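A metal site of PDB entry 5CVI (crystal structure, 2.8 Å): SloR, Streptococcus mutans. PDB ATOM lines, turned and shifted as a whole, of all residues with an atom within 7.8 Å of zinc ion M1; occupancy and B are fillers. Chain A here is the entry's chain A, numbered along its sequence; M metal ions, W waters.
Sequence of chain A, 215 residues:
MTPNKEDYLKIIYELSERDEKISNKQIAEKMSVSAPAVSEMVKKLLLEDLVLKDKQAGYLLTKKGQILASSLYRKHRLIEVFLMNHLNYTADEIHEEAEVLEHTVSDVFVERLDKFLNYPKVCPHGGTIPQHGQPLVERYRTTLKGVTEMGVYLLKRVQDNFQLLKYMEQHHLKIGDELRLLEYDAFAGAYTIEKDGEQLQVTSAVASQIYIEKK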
ATOM      1  N   TYR A  73     -26.614 -33.710  15.903  1.00  0.00           N
ATOM      2  CA  TYR A  73     -26.445 -32.271  15.772  1.00  0.00           C
ATOM      3  C   TYR A  73     -25.561 -31.916  14.582  1.00  0.00           C
ATOM      4  O   TYR A  73     -25.820 -30.936  13.872  1.00  0.00           O
ATOM      5  CB  TYR A  73     -25.897 -31.659  17.066  1.00  0.00           C
ATOM      6  CG  TYR A  73     -26.918 -31.520  18.161  1.00  0.00           C
ATOM      7  CD1 TYR A  73     -27.986 -30.636  18.039  1.00  0.00           C
ATOM      8  CD2 TYR A  73     -26.819 -32.268  19.329  1.00  0.00           C
ATOM      9  CE1 TYR A  73     -28.926 -30.507  19.041  1.00  0.00           C
ATOM     10  CE2 TYR A  73     -27.761 -32.148  20.336  1.00  0.00           C
ATOM     11  CZ  TYR A  73     -28.808 -31.260  20.187  1.00  0.00           C
ATOM     12  OH  TYR A  73     -29.749 -31.137  21.180  1.00  0.00           O
ATOM     13  N   HIS A  76     -27.727 -32.444  11.425  1.00  0.00           N
ATOM     14  CA  HIS A  76     -28.752 -31.403  11.417  1.00  0.00           C
ATOM     15  C   HIS A  76     -28.190 -30.055  11.005  1.00  0.00           C
ATOM     16  O   HIS A  76     -28.765 -29.369  10.156  1.00  0.00           O
ATOM     17  CB  HIS A  76     -29.386 -31.302  12.805  1.00  0.00           C
ATOM     18  CG  HIS A  76     -30.690 -30.562  12.811  1.00  0.00           C
ATOM     19  ND1 HIS A  76     -31.881 -31.164  12.461  1.00  0.00           N
ATOM     20  CD2 HIS A  76     -30.995 -29.288  13.143  1.00  0.00           C
ATOM     21  CE1 HIS A  76     -32.860 -30.277  12.562  1.00  0.00           C
ATOM     22  NE2 HIS A  76     -32.347 -29.140  12.978  1.00  0.00           N
ATOM     23  N   ARG A  77     -27.048 -29.696  11.585  1.00  0.00           N
ATOM     24  CA  ARG A  77     -26.480 -28.375  11.363  1.00  0.00           C
ATOM     25  C   ARG A  77     -25.814 -28.199   9.994  1.00  0.00           C
ATOM     26  O   ARG A  77     -25.942 -27.142   9.368  1.00  0.00           O
ATOM     27  CB  ARG A  77     -25.533 -27.998  12.507  1.00  0.00           C
ATOM     28  CG  ARG A  77     -26.262 -27.729  13.816  1.00  0.00           C
ATOM     29  CD  ARG A  77     -25.324 -27.409  14.961  1.00  0.00           C
ATOM     30  NE  ARG A  77     -26.073 -27.014  16.162  1.00  0.00           N
ATOM     31  CZ  ARG A  77     -25.584 -27.055  17.392  1.00  0.00           C
ATOM     32  NH1 ARG A  77     -24.346 -27.481  17.614  1.00  0.00           N
ATOM     33  NH2 ARG A  77     -26.336 -26.681  18.420  1.00  0.00           N
ATOM     34  N   LEU A  78     -25.108 -29.231   9.522  1.00  0.00           N
ATOM     35  CA  LEU A  78     -24.552 -29.182   8.167  1.00  0.00           C
ATOM     36  C   LEU A  78     -25.664 -29.040   7.137  1.00  0.00           C
ATOM     37  O   LEU A  78     -25.541 -28.283   6.178  1.00  0.00           O
ATOM     38  CB  LEU A  78     -23.706 -30.422   7.877  1.00  0.00           C
ATOM     39  CG  LEU A  78     -22.279 -30.386   8.426  1.00  0.00           C
ATOM     40  CD1 LEU A  78     -21.604 -31.742   8.289  1.00  0.00           C
ATOM     41  CD2 LEU A  78     -21.472 -29.311   7.703  1.00  0.00           C
ATOM     42  N   GLU A  80     -28.494 -27.591   7.744  1.00  0.00           N
ATOM     43  CA  GLU A  80     -29.029 -26.246   7.900  1.00  0.00           C
ATOM     44  C   GLU A  80     -28.230 -25.231   7.095  1.00  0.00           C
ATOM     45  O   GLU A  80     -28.788 -24.346   6.443  1.00  0.00           O
ATOM     46  CB  GLU A  80     -29.080 -25.832   9.372  1.00  0.00           C
ATOM     47  CG  GLU A  80     -30.198 -26.481  10.172  1.00  0.00           C
ATOM     48  CD  GLU A  80     -30.211 -26.016  11.622  1.00  0.00           C
ATOM     49  OE1 GLU A  80     -31.239 -26.220  12.303  1.00  0.00           O
ATOM     50  OE2 GLU A  80     -29.195 -25.434  12.069  1.00  0.00           O
ATOM     51  N   VAL A  81     -26.903 -25.344   7.136  1.00  0.00           N
ATOM     52  CA  VAL A  81     -26.032 -24.455   6.377  1.00  0.00           C
ATOM     53  C   VAL A  81     -26.290 -24.573   4.884  1.00  0.00           C
ATOM     54  O   VAL A  81     -26.283 -23.572   4.163  1.00  0.00           O
ATOM     55  CB  VAL A  81     -24.540 -24.740   6.646  1.00  0.00           C
ATOM     56  CG1 VAL A  81     -23.667 -23.835   5.795  1.00  0.00           C
ATOM     57  CG2 VAL A  81     -24.223 -24.564   8.112  1.00  0.00           C
ATOM     58  N   ILE A  94     -36.474 -24.395   7.677  1.00  0.00           N
ATOM     59  CA  ILE A  94     -35.325 -25.289   7.706  1.00  0.00           C
ATOM     60  C   ILE A  94     -35.437 -26.499   8.640  1.00  0.00           C
ATOM     61  O   ILE A  94     -34.811 -27.520   8.401  1.00  0.00           O
ATOM     62  CB  ILE A  94     -34.010 -24.536   8.027  1.00  0.00           C
ATOM     63  CG1 ILE A  94     -34.151 -23.793   9.357  1.00  0.00           C
ATOM     64  CG2 ILE A  94     -33.643 -23.588   6.901  1.00  0.00           C
ATOM     65  CD1 ILE A  94     -32.879 -23.113   9.819  1.00  0.00           C
ATOM     66  N   HIS A  95     -36.227 -26.380   9.705  1.00  0.00           N
ATOM     67  CA  HIS A  95     -36.234 -27.427  10.721  1.00  0.00           C
ATOM     68  C   HIS A  95     -36.787 -28.763  10.239  1.00  0.00           C
ATOM     69  O   HIS A  95     -36.081 -29.776  10.268  1.00  0.00           O
ATOM     70  CB  HIS A  95     -36.959 -27.003  11.996  1.00  0.00           C
ATOM     71  CG  HIS A  95     -36.903 -28.032  13.077  1.00  0.00           C
ATOM     72  ND1 HIS A  95     -35.726 -28.369  13.705  1.00  0.00           N
ATOM     73  CD2 HIS A  95     -37.866 -28.810  13.627  1.00  0.00           C
ATOM     74  CE1 HIS A  95     -35.958 -29.314  14.597  1.00  0.00           C
ATOM     75  NE2 HIS A  95     -37.255 -29.594  14.577  1.00  0.00           N
ATOM     76  N   VAL A 122     -19.985 -23.117  12.432  1.00  0.00           N
ATOM     77  CA  VAL A 122     -21.212 -22.828  13.176  1.00  0.00           C
ATOM     78  C   VAL A 122     -22.422 -22.921  12.258  1.00  0.00           C
ATOM     79  O   VAL A 122     -22.313 -22.674  11.055  1.00  0.00           O
ATOM     80  CB  VAL A 122     -21.166 -21.424  13.833  1.00  0.00           C
ATOM     81  CG1 VAL A 122     -19.731 -21.019  14.117  1.00  0.00           C
ATOM     82  CG2 VAL A 122     -21.841 -20.390  12.950  1.00  0.00           C
ATOM     83  N   CYS A 123     -23.564 -23.279  12.830  1.00  0.00           N
ATOM     84  CA  CYS A 123     -24.809 -23.328  12.075  1.00  0.00           C
ATOM     85  C   CYS A 123     -25.527 -21.991  12.227  1.00  0.00           C
ATOM     86  O   CYS A 123     -25.091 -21.138  12.992  1.00  0.00           O
ATOM     87  CB  CYS A 123     -25.704 -24.464  12.575  1.00  0.00           C
ATOM     88  SG  CYS A 123     -26.697 -24.057  14.045  1.00  0.00           S
ATOM     89  N   PRO A 124     -26.637 -21.813  11.490  1.00  0.00           N
ATOM     90  CA  PRO A 124     -27.452 -20.588  11.531  1.00  0.00           C
ATOM     91  C   PRO A 124     -27.818 -20.117  12.936  1.00  0.00           C
ATOM     92  O   PRO A 124     -28.022 -18.923  13.143  1.00  0.00           O
ATOM     93  CB  PRO A 124     -28.712 -21.001  10.771  1.00  0.00           C
ATOM     94  CG  PRO A 124     -28.232 -22.028   9.802  1.00  0.00           C
ATOM     95  CD  PRO A 124     -27.150 -22.784  10.510  1.00  0.00           C
ATOM     96  N   HIS A 125     -27.885 -21.032  13.902  1.00  0.00           N
ATOM     97  CA  HIS A 125     -28.244 -20.657  15.269  1.00  0.00           C
ATOM     98  C   HIS A 125     -27.028 -20.259  16.088  1.00  0.00           C
ATOM     99  O   HIS A 125     -27.156 -19.840  17.237  1.00  0.00           O
ATOM    100  CB  HIS A 125     -28.991 -21.801  15.971  1.00  0.00           C
ATOM    101  CG  HIS A 125     -30.227 -22.256  15.246  1.00  0.00           C
ATOM    102  ND1 HIS A 125     -30.214 -23.288  14.341  1.00  0.00           N
ATOM    103  CD2 HIS A 125     -31.507 -21.821  15.302  1.00  0.00           C
ATOM    104  CE1 HIS A 125     -31.432 -23.473  13.874  1.00  0.00           C
ATOM    105  NE2 HIS A 125     -32.233 -22.591  14.442  1.00  0.00           N
ATOM    106  N   GLY A 126     -25.848 -20.385  15.485  1.00  0.00           N
ATOM    107  CA  GLY A 126     -24.611 -20.126  16.198  1.00  0.00           C
ATOM    108  C   GLY A 126     -24.091 -21.393  16.870  1.00  0.00           C
ATOM    109  O   GLY A 126     -23.141 -21.352  17.654  1.00  0.00           O
ATOM    110  N   GLY A 127     -24.735 -22.515  16.561  1.00  0.00           N
ATOM    111  CA  GLY A 127     -24.348 -23.793  17.122  1.00  0.00           C
ATOM    112  C   GLY A 127     -23.091 -24.351  16.488  1.00  0.00           C
ATOM    113  O   GLY A 127     -22.906 -24.267  15.270  1.00  0.00           O
ATOM    114  N   THR A 128     -22.214 -24.918  17.300  1.00  0.00           N
ATOM    115  CA  THR A 128     -20.947 -25.465  16.822  1.00  0.00           C
ATOM    116  C   THR A 128     -21.148 -26.763  16.045  1.00  0.00           C
ATOM    117  O   THR A 128     -21.966 -27.596  16.406  1.00  0.00           O
ATOM    118  CB  THR A 128     -19.966 -25.727  17.991  1.00  0.00           C
ATOM    119  OG1 THR A 128     -19.652 -24.492  18.633  1.00  0.00           O
ATOM    120  CG2 THR A 128     -18.681 -26.353  17.465  1.00  0.00           C
ATOM    121  N   ILE A 129     -20.384 -26.920  14.970  1.00  0.00           N
ATOM    122  CA  ILE A 129     -20.433 -28.151  14.187  1.00  0.00           C
ATOM    123  C   ILE A 129     -19.200 -29.007  14.477  1.00  0.00           C
ATOM    124  O   ILE A 129     -18.083 -28.673  14.073  1.00  0.00           O
ATOM    125  CB  ILE A 129     -20.535 -27.846  12.676  1.00  0.00           C
ATOM    126  CG1 ILE A 129     -21.767 -26.985  12.395  1.00  0.00           C
ATOM    127  CG2 ILE A 129     -20.603 -29.143  11.876  1.00  0.00           C
ATOM    128  CD1 ILE A 129     -21.986 -26.648  10.944  1.00  0.00           C
ATOM    129  N   VAL A 158     -28.365 -19.197  19.703  1.00  0.00           N
ATOM    130  CA  VAL A 158     -29.723 -19.386  20.169  1.00  0.00           C
ATOM    131  C   VAL A 158     -30.126 -20.849  20.042  1.00  0.00           C
ATOM    132  O   VAL A 158     -29.505 -21.595  19.280  1.00  0.00           O
ATOM    133  CB  VAL A 158     -30.726 -18.511  19.384  1.00  0.00           C
ATOM    134  CG1 VAL A 158     -30.443 -17.039  19.632  1.00  0.00           C
ATOM    135  CG2 VAL A 158     -30.660 -18.828  17.901  1.00  0.00           C
ATOM    136  N   GLN A 159     -31.136 -21.259  20.797  1.00  0.00           N
ATOM    137  CA  GLN A 159     -31.655 -22.616  20.699  1.00  0.00           C
ATOM    138  C   GLN A 159     -32.437 -22.780  19.403  1.00  0.00           C
ATOM    139  O   GLN A 159     -33.026 -21.826  18.898  1.00  0.00           O
ATOM    140  CB  GLN A 159     -32.585 -22.939  21.873  1.00  0.00           C
ATOM    141  CG  GLN A 159     -31.881 -23.155  23.202  1.00  0.00           C
ATOM    142  CD  GLN A 159     -31.185 -24.493  23.296  1.00  0.00           C
ATOM    143  OE1 GLN A 159     -30.866 -25.116  22.288  1.00  0.00           O
ATOM    144  NE2 GLN A 159     -30.952 -24.953  24.527  1.00  0.00           N
ATOM    145  N   ASP A 160     -32.414 -23.990  18.871  1.00  0.00           N
ATOM    146  CA  ASP A 160     -33.292 -24.369  17.780  1.00  0.00           C
ATOM    147  C   ASP A 160     -34.693 -24.501  18.368  1.00  0.00           C
ATOM    148  O   ASP A 160     -35.038 -25.539  18.940  1.00  0.00           O
ATOM    149  CB  ASP A 160     -32.842 -25.702  17.193  1.00  0.00           C
ATOM    150  CG  ASP A 160     -33.518 -26.033  15.883  1.00  0.00           C
ATOM    151  OD1 ASP A 160     -34.594 -25.477  15.606  1.00  0.00           O
ATOM    152  OD2 ASP A 160     -32.959 -26.856  15.136  1.00  0.00           O
HETATM  153 ZN    ZN M   1     -28.840 -24.851  13.966  1.00  0.00          ZN
HETATM  154 ZN    ZN M   2     -33.773 -27.838  13.629  1.00  0.00          ZN
HETATM  155  O   HOH W   1     -29.213 -26.457  15.913  1.00  0.00           O
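The side-chain carboxylate of Glu 80 sits close to a ring nitrogen (NE2) of His 76 (3.2 Å).
The backbone NH (N) of Val 158 sits at hydrogen-bond distance from the backbone carbonyl oxygen (O) of His 125 (2.8 Å).
SG of Cys 123 sits close to NE of Arg 77 (3.7 Å).
The side-chain sulfur of Cys 123 sits close to the backbone NH of Gly 127, at 3.5 Å.
The guanidinium group (NH1) of Arg 77 lies within hydrogen-bond range of the backbone carbonyl oxygen (O) of Thr 128 (2.7 Å).
Arg 77 touches zinc ion M1 (CG to ZN, 3.9 Å).
Four residues have an atom within 4 Å of zinc ion M1: Arg 77, Glu 80, Cys 123 and His 125.
The nearest printed residue that does not touch zinc ion M1 is Pro 124 (4.4 Å).
Zinc ion M1 is bound by OE2 of Glu 80 (2.0 Å), ND1 of His 125 (2.1 Å), SG of Cys 123 (2.3 Å) and water W1 (2.6 Å).
Zinc ion M1 has four donor atoms within binding distance.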
